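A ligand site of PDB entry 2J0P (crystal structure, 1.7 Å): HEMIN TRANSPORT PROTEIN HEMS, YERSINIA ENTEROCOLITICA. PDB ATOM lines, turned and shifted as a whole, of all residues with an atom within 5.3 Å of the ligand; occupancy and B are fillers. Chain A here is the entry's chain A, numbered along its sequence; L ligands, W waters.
The side-chain amide oxygen (OE1) of Gln 316 sits close to an oxygen (O4) of the ligand, 3.1 Å away.
The guanidinium group (NH1) of Arg 321 lies within salt-bridge range of an oxygen (O2) of the ligand (2.8 Å).
The guanidinium group of Arg 209 is in salt-bridge range of an oxygen (O3) of the ligand (2.9 Å).
NZ of Lys 294 lies within salt-bridge range of O4 of the ligand (3.2 Å).
The side-chain hydroxyl (OH) of Tyr 318 sits at hydrogen-bond distance from an oxygen (O4) of the ligand, 2.8 Å away.
FE1 of the ligand is bound by NE2 of His 196 (2.0 Å).
N of Phe 246 is in hydrogen-bond range of O of Gln 316, at 2.8 Å.
The side-chain carboxylate of Glu 305 lies within salt-bridge range of the guanidinium group of Arg 209, at 2.7 Å.
The side-chain amide oxygen of Gln 316 is in hydrogen-bond range of the side-chain hydroxyl of Ser 303, 3.4 Å away.
The side-chain amide oxygen of Gln 316 sits close to the side-chain carboxylate of Glu 305, 3.4 Å away.
The backbone NH (N) of Gly 91 lies within hydrogen-bond range of the backbone carbonyl oxygen (O) of Leu 103.
The backbone NH (N) of Arg 102 lies within hydrogen-bond range of the backbone carbonyl oxygen (O) of Val 253 (2.9 Å).
The backbone NH (N) of Met 244 sits at hydrogen-bond distance from the backbone carbonyl oxygen (O) of Tyr 318 (2.8 Å).
NZ of Lys 294 is in salt-bridge range of OE2 of Glu 305, at 3.0 Å.
The guanidinium group of Arg 102 lies close to a nitrogen (N3) of the ligand (3.3 Å).
Residues that only touch the ligand: Phe 199 (3.4 Å), Phe 246 (3.5 Å), Val 301 (3.6 Å), Gly 91 (3.6 Å), Leu 92 (3.6 Å), Ala 90 (3.6 Å), Leu 103 (3.7 Å), Val 195 (3.9 Å) and Phe 104 (3.9 Å).
Hydrophobic or aromatic side chains within 4 Å of the ligand: Ala 90, Leu 92, Phe 104, Val 195, His 196, Phe 199, Phe 246, Val 301 and Tyr 318.
Of the 25 residues printed, 16 come within 4 Å of the ligand.
The nearest printed residue that does not touch the ligand is Phe 198 (4.05 Å).
Water W1 bridges O1 of the ligand (2.6 Å) and O of Gly 319 (2.9 Å).
Water W2 lies within hydrogen-bond range of the guanidinium group of Arg 209, an oxygen (O3) of the ligand and the side-chain amide nitrogen of Gln 316.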
ATOM      1  N   ALA A  90     -34.634   0.263   8.227  1.00  0.00           N
ATOM      2  CA  ALA A  90     -34.025  -0.879   8.854  1.00  0.00           C
ATOM      3  C   ALA A  90     -34.053  -0.730  10.357  1.00  0.00           C
ATOM      4  O   ALA A  90     -33.314   0.005  10.913  1.00  0.00           O
ATOM      5  CB  ALA A  90     -32.697  -1.058   8.384  1.00  0.00           C
ATOM      6  N   GLY A  91     -34.951  -1.448  10.989  1.00  0.00           N
ATOM      7  CA  GLY A  91     -35.119  -1.357  12.406  1.00  0.00           C
ATOM      8  C   GLY A  91     -34.580  -2.484  13.229  1.00  0.00           C
ATOM      9  O   GLY A  91     -34.355  -3.513  12.744  1.00  0.00           O
ATOM     10  N   LEU A  92     -34.347  -2.215  14.476  1.00  0.00           N
ATOM     11  CA  LEU A  92     -33.912  -3.230  15.375  1.00  0.00           C
ATOM     12  C   LEU A  92     -34.513  -3.223  16.740  1.00  0.00           C
ATOM     13  O   LEU A  92     -34.882  -2.248  17.244  1.00  0.00           O
ATOM     14  CB  LEU A  92     -32.417  -3.394  15.436  1.00  0.00           C
ATOM     15  CG  LEU A  92     -31.562  -2.196  15.646  1.00  0.00           C
ATOM     16  CD1 LEU A  92     -30.247  -2.582  16.196  1.00  0.00           C
ATOM     17  CD2 LEU A  92     -31.424  -1.406  14.445  1.00  0.00           C
ATOM     18  N   LEU A  94     -32.979  -4.900  19.793  1.00  0.00           N
ATOM     19  CA  LEU A  94     -31.705  -5.444  20.100  1.00  0.00           C
ATOM     20  C   LEU A  94     -31.552  -6.081  21.458  1.00  0.00           C
ATOM     21  O   LEU A  94     -31.233  -5.448  22.373  1.00  0.00           O
ATOM     22  CB  LEU A  94     -30.682  -4.351  19.909  1.00  0.00           C
ATOM     23  CG  LEU A  94     -29.245  -4.737  20.117  1.00  0.00           C
ATOM     24  CD1 LEU A  94     -28.891  -5.790  19.132  1.00  0.00           C
ATOM     25  CD2 LEU A  94     -28.416  -3.511  19.862  1.00  0.00           C
ATOM     26  N   ARG A 102     -34.746  -7.998  13.552  1.00  0.00           N
ATOM     27  CA  ARG A 102     -34.295  -7.115  12.523  1.00  0.00           C
ATOM     28  C   ARG A 102     -35.492  -6.893  11.623  1.00  0.00           C
ATOM     29  O   ARG A 102     -36.074  -7.806  11.161  1.00  0.00           O
ATOM     30  CB  ARG A 102     -33.140  -7.712  11.775  1.00  0.00           C
ATOM     31  CG  ARG A 102     -32.014  -8.088  12.665  1.00  0.00           C
ATOM     32  CD  ARG A 102     -31.441  -6.918  13.399  1.00  0.00           C
ATOM     33  NE  ARG A 102     -30.303  -7.314  14.161  1.00  0.00           N
ATOM     34  CZ  ARG A 102     -30.281  -7.609  15.434  1.00  0.00           C
ATOM     35  NH1 ARG A 102     -29.162  -7.983  15.971  1.00  0.00           N
ATOM     36  NH2 ARG A 102     -31.341  -7.513  16.194  1.00  0.00           N
ATOM     37  N   LEU A 103     -35.860  -5.638  11.466  1.00  0.00           N
ATOM     38  CA  LEU A 103     -37.029  -5.245  10.734  1.00  0.00           C
ATOM     39  C   LEU A 103     -36.886  -4.429   9.467  1.00  0.00           C
ATOM     40  O   LEU A 103     -36.188  -3.517   9.442  1.00  0.00           O
ATOM     41  CB  LEU A 103     -37.968  -4.487  11.667  1.00  0.00           C
ATOM     42  CG  LEU A 103     -38.071  -4.992  13.086  1.00  0.00           C
ATOM     43  CD1 LEU A 103     -38.769  -4.049  13.909  1.00  0.00           C
ATOM     44  CD2 LEU A 103     -38.888  -6.169  13.059  1.00  0.00           C
ATOM     45  N   PHE A 104     -37.625  -4.779   8.448  1.00  0.00           N
ATOM     46  CA  PHE A 104     -37.612  -4.021   7.229  1.00  0.00           C
ATOM     47  C   PHE A 104     -38.971  -3.411   7.160  1.00  0.00           C
ATOM     48  O   PHE A 104     -39.853  -3.924   6.575  1.00  0.00           O
ATOM     49  CB  PHE A 104     -37.264  -4.865   6.040  1.00  0.00           C
ATOM     50  CG  PHE A 104     -35.992  -5.588   6.191  1.00  0.00           C
ATOM     51  CD1 PHE A 104     -34.828  -5.027   5.798  1.00  0.00           C
ATOM     52  CD2 PHE A 104     -35.950  -6.802   6.765  1.00  0.00           C
ATOM     53  CE1 PHE A 104     -33.679  -5.665   5.949  1.00  0.00           C
ATOM     54  CE2 PHE A 104     -34.788  -7.458   6.925  1.00  0.00           C
ATOM     55  CZ  PHE A 104     -33.651  -6.899   6.524  1.00  0.00           C
ATOM     56  N   ASP A 194     -18.293  -5.185   5.768  1.00  0.00           N
ATOM     57  CA  ASP A 194     -19.165  -5.728   6.762  1.00  0.00           C
ATOM     58  C   ASP A 194     -20.322  -6.518   6.152  1.00  0.00           C
ATOM     59  O   ASP A 194     -20.785  -6.209   5.075  1.00  0.00           O
ATOM     60  CB  ASP A 194     -19.653  -4.651   7.698  1.00  0.00           C
ATOM     61  CG  ASP A 194     -20.511  -5.208   8.769  1.00  0.00           C
ATOM     62  OD1 ASP A 194     -20.019  -6.031   9.528  1.00  0.00           O
ATOM     63  OD2 ASP A 194     -21.693  -4.888   8.796  1.00  0.00           O
ATOM     64  N   VAL A 195     -20.797  -7.537   6.855  1.00  0.00           N
ATOM     65  CA  VAL A 195     -21.864  -8.334   6.314  1.00  0.00           C
ATOM     66  C   VAL A 195     -23.079  -7.558   5.948  1.00  0.00           C
ATOM     67  O   VAL A 195     -23.712  -7.841   4.963  1.00  0.00           O
ATOM     68  CB  VAL A 195     -22.276  -9.529   7.147  1.00  0.00           C
ATOM     69  CG1 VAL A 195     -21.178 -10.434   7.383  1.00  0.00           C
ATOM     70  CG2 VAL A 195     -22.902  -9.103   8.413  1.00  0.00           C
ATOM     71  N   HIS A 196     -23.418  -6.576   6.757  1.00  0.00           N
ATOM     72  CA  HIS A 196     -24.587  -5.792   6.481  1.00  0.00           C
ATOM     73  C   HIS A 196     -24.605  -5.124   5.090  1.00  0.00           C
ATOM     74  O   HIS A 196     -25.619  -4.701   4.637  1.00  0.00           O
ATOM     75  CB  HIS A 196     -24.960  -4.861   7.641  1.00  0.00           C
ATOM     76  CG  HIS A 196     -25.190  -5.587   8.934  1.00  0.00           C
ATOM     77  ND1 HIS A 196     -24.194  -5.823   9.840  1.00  0.00           N
ATOM     78  CD2 HIS A 196     -26.300  -6.164   9.440  1.00  0.00           C
ATOM     79  CE1 HIS A 196     -24.690  -6.503  10.860  1.00  0.00           C
ATOM     80  NE2 HIS A 196     -25.968  -6.719  10.640  1.00  0.00           N
ATOM     81  N   PHE A 198     -24.177  -6.689   2.321  1.00  0.00           N
ATOM     82  CA  PHE A 198     -24.644  -7.671   1.387  1.00  0.00           C
ATOM     83  C   PHE A 198     -25.988  -7.330   0.770  1.00  0.00           C
ATOM     84  O   PHE A 198     -26.170  -7.550  -0.389  1.00  0.00           O
ATOM     85  CB  PHE A 198     -24.593  -9.065   2.030  1.00  0.00           C
ATOM     86  CG  PHE A 198     -24.804 -10.199   1.085  1.00  0.00           C
ATOM     87  CD1 PHE A 198     -25.878 -10.999   1.205  1.00  0.00           C
ATOM     88  CD2 PHE A 198     -23.917 -10.495   0.103  1.00  0.00           C
ATOM     89  CE1 PHE A 198     -26.095 -12.029   0.402  1.00  0.00           C
ATOM     90  CE2 PHE A 198     -24.142 -11.539  -0.716  1.00  0.00           C
ATOM     91  CZ  PHE A 198     -25.238 -12.308  -0.556  1.00  0.00           C
ATOM     92  N   PHE A 199     -26.934  -6.808   1.527  1.00  0.00           N
ATOM     93  CA  PHE A 199     -28.238  -6.479   0.948  1.00  0.00           C
ATOM     94  C   PHE A 199     -28.146  -5.453  -0.163  1.00  0.00           C
ATOM     95  O   PHE A 199     -28.790  -5.589  -1.141  1.00  0.00           O
ATOM     96  CB  PHE A 199     -29.282  -6.015   1.977  1.00  0.00           C
ATOM     97  CG  PHE A 199     -29.137  -6.632   3.336  1.00  0.00           C
ATOM     98  CD1 PHE A 199     -29.125  -5.839   4.472  1.00  0.00           C
ATOM     99  CD2 PHE A 199     -29.017  -7.973   3.493  1.00  0.00           C
ATOM    100  CE1 PHE A 199     -28.961  -6.380   5.712  1.00  0.00           C
ATOM    101  CE2 PHE A 199     -28.871  -8.512   4.743  1.00  0.00           C
ATOM    102  CZ  PHE A 199     -28.841  -7.717   5.845  1.00  0.00           C
ATOM    103  N   ARG A 209     -30.116 -14.329  -3.514  1.00  0.00           N
ATOM    104  CA  ARG A 209     -29.012 -14.836  -2.745  1.00  0.00           C
ATOM    105  C   ARG A 209     -28.390 -15.998  -3.503  1.00  0.00           C
ATOM    106  O   ARG A 209     -27.229 -16.017  -3.654  1.00  0.00           O
ATOM    107  CB  ARG A 209     -29.463 -15.299  -1.358  1.00  0.00           C
ATOM    108  CG  ARG A 209     -29.950 -14.193  -0.474  1.00  0.00           C
ATOM    109  CD  ARG A 209     -30.188 -14.569   0.955  1.00  0.00           C
ATOM    110  NE  ARG A 209     -28.935 -14.812   1.634  1.00  0.00           N
ATOM    111  CZ  ARG A 209     -28.289 -13.936   2.392  1.00  0.00           C
ATOM    112  NH1 ARG A 209     -27.170 -14.271   2.966  1.00  0.00           N
ATOM    113  NH2 ARG A 209     -28.781 -12.726   2.564  1.00  0.00           N
ATOM    114  N   MET A 244     -25.936 -18.920  16.430  1.00  0.00           N
ATOM    115  CA  MET A 244     -27.030 -18.004  16.109  1.00  0.00           C
ATOM    116  C   MET A 244     -27.897 -18.642  15.070  1.00  0.00           C
ATOM    117  O   MET A 244     -27.407 -19.143  14.182  1.00  0.00           O
ATOM    118  CB  MET A 244     -26.490 -16.722  15.488  1.00  0.00           C
ATOM    119  CG  MET A 244     -25.643 -15.942  16.380  1.00  0.00           C
ATOM    120  SD  MET A 244     -24.911 -14.486  15.643  1.00  0.00           S
ATOM    121  CE  MET A 244     -26.313 -13.458  15.599  1.00  0.00           C
ATOM    122  N   PHE A 246     -31.006 -17.683  12.443  1.00  0.00           N
ATOM    123  CA  PHE A 246     -31.794 -16.609  11.903  1.00  0.00           C
ATOM    124  C   PHE A 246     -32.948 -17.205  11.111  1.00  0.00           C
ATOM    125  O   PHE A 246     -32.729 -18.009  10.305  1.00  0.00           O
ATOM    126  CB  PHE A 246     -30.996 -15.816  10.871  1.00  0.00           C
ATOM    127  CG  PHE A 246     -29.878 -14.950  11.405  1.00  0.00           C
ATOM    128  CD1 PHE A 246     -29.813 -13.639  11.086  1.00  0.00           C
ATOM    129  CD2 PHE A 246     -28.847 -15.472  12.100  1.00  0.00           C
ATOM    130  CE1 PHE A 246     -28.828 -12.876  11.517  1.00  0.00           C
ATOM    131  CE2 PHE A 246     -27.849 -14.683  12.506  1.00  0.00           C
ATOM    132  CZ  PHE A 246     -27.842 -13.406  12.215  1.00  0.00           C
ATOM    133  N   VAL A 253     -36.753 -10.594  10.522  1.00  0.00           N
ATOM    134  CA  VAL A 253     -35.782 -11.623  10.830  1.00  0.00           C
ATOM    135  C   VAL A 253     -35.631 -11.681  12.341  1.00  0.00           C
ATOM    136  O   VAL A 253     -35.352 -10.737  12.956  1.00  0.00           O
ATOM    137  CB  VAL A 253     -34.426 -11.370  10.183  1.00  0.00           C
ATOM    138  CG1 VAL A 253     -33.492 -12.535  10.389  1.00  0.00           C
ATOM    139  CG2 VAL A 253     -34.586 -11.161   8.748  1.00  0.00           C
ATOM    140  N   LYS A 294     -18.307 -14.061   4.365  1.00  0.00           N
ATOM    141  CA  LYS A 294     -18.422 -12.655   4.133  1.00  0.00           C
ATOM    142  C   LYS A 294     -17.473 -11.892   5.009  1.00  0.00           C
ATOM    143  O   LYS A 294     -17.292 -12.218   6.113  1.00  0.00           O
ATOM    144  CB  LYS A 294     -19.858 -12.221   4.363  1.00  0.00           C
ATOM    145  CG  LYS A 294     -20.810 -12.947   3.515  1.00  0.00           C
ATOM    146  CD  LYS A 294     -22.215 -12.481   3.709  1.00  0.00           C
ATOM    147  CE  LYS A 294     -23.172 -13.286   2.962  1.00  0.00           C
ATOM    148  NZ  LYS A 294     -23.531 -14.489   3.677  1.00  0.00           N
ATOM    149  N   THR A 296     -15.563  -8.974   7.284  1.00  0.00           N
ATOM    150  CA  THR A 296     -15.825  -8.027   8.347  1.00  0.00           C
ATOM    151  C   THR A 296     -14.545  -7.472   8.931  1.00  0.00           C
ATOM    152  O   THR A 296     -13.499  -8.007   8.758  1.00  0.00           O
ATOM    153  CB  THR A 296     -16.700  -8.533   9.462  1.00  0.00           C
ATOM    154  OG1 THR A 296     -15.936  -9.105  10.493  1.00  0.00           O
ATOM    155  CG2 THR A 296     -17.695  -9.503   8.977  1.00  0.00           C
ATOM    156  N   VAL A 301     -16.675 -14.129   8.365  1.00  0.00           N
ATOM    157  CA  VAL A 301     -17.710 -14.811   9.096  1.00  0.00           C
ATOM    158  C   VAL A 301     -18.348 -15.824   8.144  1.00  0.00           C
ATOM    159  O   VAL A 301     -18.584 -15.544   7.010  1.00  0.00           O
ATOM    160  CB  VAL A 301     -18.728 -13.892   9.736  1.00  0.00           C
ATOM    161  CG1 VAL A 301     -18.064 -13.124  10.785  1.00  0.00           C
ATOM    162  CG2 VAL A 301     -19.332 -13.014   8.761  1.00  0.00           C
ATOM    163  N   SER A 303     -21.329 -18.666   7.308  1.00  0.00           N
ATOM    164  CA  SER A 303     -22.650 -19.179   7.670  1.00  0.00           C
ATOM    165  C   SER A 303     -23.168 -20.294   6.826  1.00  0.00           C
ATOM    166  O   SER A 303     -22.754 -20.507   5.754  1.00  0.00           O
ATOM    167  CB  SER A 303     -23.692 -18.097   7.677  1.00  0.00           C
ATOM    168  OG  SER A 303     -23.958 -17.723   6.412  1.00  0.00           O
ATOM    169  N   GLU A 305     -26.425 -21.432   5.019  1.00  0.00           N
ATOM    170  CA  GLU A 305     -27.657 -20.920   4.489  1.00  0.00           C
ATOM    171  C   GLU A 305     -28.476 -21.954   3.787  1.00  0.00           C
ATOM    172  O   GLU A 305     -27.990 -22.592   2.930  1.00  0.00           O
ATOM    173  CB  GLU A 305     -27.416 -19.716   3.583  1.00  0.00           C
ATOM    174  CG  GLU A 305     -26.469 -18.732   4.124  1.00  0.00           C
ATOM    175  CD  GLU A 305     -26.605 -17.349   3.563  1.00  0.00           C
ATOM    176  OE1 GLU A 305     -27.686 -16.939   3.183  1.00  0.00           O
ATOM    177  OE2 GLU A 305     -25.613 -16.631   3.527  1.00  0.00           O
ATOM    178  N   GLN A 316     -30.725 -19.478   8.431  1.00  0.00           N
ATOM    179  CA  GLN A 316     -29.303 -19.310   8.367  1.00  0.00           C
ATOM    180  C   GLN A 316     -28.652 -19.353   9.725  1.00  0.00           C
ATOM    181  O   GLN A 316     -29.188 -18.918  10.675  1.00  0.00           O
ATOM    182  CB  GLN A 316     -28.903 -18.172   7.459  1.00  0.00           C
ATOM    183  CG  GLN A 316     -28.332 -17.036   8.086  1.00  0.00           C
ATOM    184  CD  GLN A 316     -27.916 -15.945   7.111  1.00  0.00           C
ATOM    185  OE1 GLN A 316     -26.811 -15.949   6.619  1.00  0.00           O
ATOM    186  NE2 GLN A 316     -28.785 -15.004   6.873  1.00  0.00           N
ATOM    187  N   TYR A 318     -24.997 -18.989  12.134  1.00  0.00           N
ATOM    188  CA  TYR A 318     -23.719 -18.362  12.311  1.00  0.00           C
ATOM    189  C   TYR A 318     -23.273 -18.749  13.714  1.00  0.00           C
ATOM    190  O   TYR A 318     -23.986 -19.266  14.434  1.00  0.00           O
ATOM    191  CB  TYR A 318     -23.882 -16.854  12.337  1.00  0.00           C
ATOM    192  CG  TYR A 318     -23.701 -16.120  11.034  1.00  0.00           C
ATOM    193  CD1 TYR A 318     -24.743 -15.511  10.406  1.00  0.00           C
ATOM    194  CD2 TYR A 318     -22.478 -16.013  10.454  1.00  0.00           C
ATOM    195  CE1 TYR A 318     -24.567 -14.846   9.247  1.00  0.00           C
ATOM    196  CE2 TYR A 318     -22.307 -15.369   9.337  1.00  0.00           C
ATOM    197  CZ  TYR A 318     -23.322 -14.778   8.722  1.00  0.00           C
ATOM    198  OH  TYR A 318     -23.084 -14.132   7.580  1.00  0.00           O
ATOM    199  N   GLY A 319     -22.050 -18.464  14.053  1.00  0.00           N
ATOM    200  CA  GLY A 319     -21.601 -18.725  15.381  1.00  0.00           C
ATOM    201  C   GLY A 319     -21.772 -17.427  16.148  1.00  0.00           C
ATOM    202  O   GLY A 319     -21.779 -16.397  15.582  1.00  0.00           O
ATOM    203  N   ARG A 321     -20.968 -14.202  17.997  1.00  0.00           N
ATOM    204  CA  ARG A 321     -19.864 -13.269  17.878  1.00  0.00           C
ATOM    205  C   ARG A 321     -20.223 -11.875  18.331  1.00  0.00           C
ATOM    206  O   ARG A 321     -21.283 -11.433  18.095  1.00  0.00           O
ATOM    207  CB  ARG A 321     -19.444 -13.148  16.431  1.00  0.00           C
ATOM    208  CG  ARG A 321     -18.155 -12.502  16.242  1.00  0.00           C
ATOM    209  CD  ARG A 321     -17.769 -12.466  14.819  1.00  0.00           C
ATOM    210  NE  ARG A 321     -18.454 -11.490  14.038  1.00  0.00           N
ATOM    211  CZ  ARG A 321     -18.111 -10.235  13.953  1.00  0.00           C
ATOM    212  NH1 ARG A 321     -18.791  -9.426  13.205  1.00  0.00           N
ATOM    213  NH2 ARG A 321     -17.082  -9.801  14.651  1.00  0.00           N
HETATM  214  C1  LIG L   1     -25.882 -10.590  10.498  1.00  0.00           C
HETATM  215  C2  LIG L   1     -25.240  -8.289  14.753  1.00  0.00           C
HETATM  216  C3  LIG L   1     -27.909  -4.684  12.888  1.00  0.00           C
HETATM  217  C4  LIG L   1     -29.855  -7.814   9.722  1.00  0.00           C
HETATM  218  C5  LIG L   1     -25.419 -10.271  11.762  1.00  0.00           C
HETATM  219  C6  LIG L   1     -24.447 -11.019  12.538  1.00  0.00           C
HETATM  220  C7  LIG L   1     -24.237 -10.378  13.705  1.00  0.00           C
HETATM  221  C8  LIG L   1     -25.116  -9.215  13.724  1.00  0.00           C
HETATM  222  C9  LIG L   1     -23.301 -10.798  14.879  1.00  0.00           C
HETATM  223  C10 LIG L   1     -23.727 -12.300  12.030  1.00  0.00           C
HETATM  224  C11 LIG L   1     -22.548 -11.879  11.119  1.00  0.00           C
HETATM  225  C12 LIG L   1     -21.370 -11.375  11.917  1.00  0.00           C
HETATM  226  O1  LIG L   1     -20.848 -12.108  12.802  1.00  0.00           O
HETATM  227  O2  LIG L   1     -20.984 -10.194  11.734  1.00  0.00           O
HETATM  228  C13 LIG L   1     -25.886  -7.065  14.612  1.00  0.00           C
HETATM  229  C14 LIG L   1     -25.747  -5.917  15.477  1.00  0.00           C
HETATM  230  C15 LIG L   1     -26.501  -4.925  14.982  1.00  0.00           C
HETATM  231  C16 LIG L   1     -27.105  -5.399  13.746  1.00  0.00           C
HETATM  232  C17 LIG L   1     -24.902  -5.867  16.769  1.00  0.00           C
HETATM  233  C18 LIG L   1     -26.674  -3.523  15.624  1.00  0.00           C
HETATM  234  C19 LIG L   1     -26.489  -2.453  14.845  1.00  0.00           C
HETATM  235  C20 LIG L   1     -28.688  -5.204  11.880  1.00  0.00           C
HETATM  236  C21 LIG L   1     -29.805  -4.553  11.203  1.00  0.00           C
HETATM  237  C22 LIG L   1     -30.336  -5.427  10.336  1.00  0.00           C
HETATM  238  C23 LIG L   1     -29.601  -6.663  10.433  1.00  0.00           C
HETATM  239  C24 LIG L   1     -30.299  -3.103  11.439  1.00  0.00           C
HETATM  240  C25 LIG L   1     -31.552  -5.237   9.384  1.00  0.00           C
HETATM  241  C26 LIG L   1     -32.581  -4.438   9.722  1.00  0.00           C
HETATM  242  C27 LIG L   1     -28.969  -8.864   9.618  1.00  0.00           C
HETATM  243  C28 LIG L   1     -29.050  -9.935   8.648  1.00  0.00           C
HETATM  244  C29 LIG L   1     -27.807 -10.786   8.910  1.00  0.00           C
HETATM  245  C30 LIG L   1     -27.061 -10.124   9.950  1.00  0.00           C
HETATM  246  C31 LIG L   1     -30.172 -10.272   7.645  1.00  0.00           C
HETATM  247  C32 LIG L   1     -27.357 -12.008   8.095  1.00  0.00           C
HETATM  248  C33 LIG L   1     -26.372 -11.419   7.089  1.00  0.00           C
HETATM  249  C34 LIG L   1     -26.124 -12.381   5.956  1.00  0.00           C
HETATM  250  O3  LIG L   1     -26.837 -12.227   4.940  1.00  0.00           O
HETATM  251  O4  LIG L   1     -25.233 -13.279   6.069  1.00  0.00           O
HETATM  252  N1  LIG L   1     -25.824  -9.185  12.525  1.00  0.00           N
HETATM  253  N2  LIG L   1     -26.683  -6.714  13.553  1.00  0.00           N
HETATM  254  N3  LIG L   1     -28.604  -6.507  11.392  1.00  0.00           N
HETATM  255  N4  LIG L   1     -27.780  -8.983  10.339  1.00  0.00           N
HETATM  256 FE1  LIG L   1     -27.087  -7.768  11.909  1.00  0.00          FE
HETATM  257  O   HOH W   1     -20.923 -14.669  13.442  1.00  0.00           O
HETATM  258  O   HOH W   2     -29.598 -12.777   4.863  1.00  0.00           O
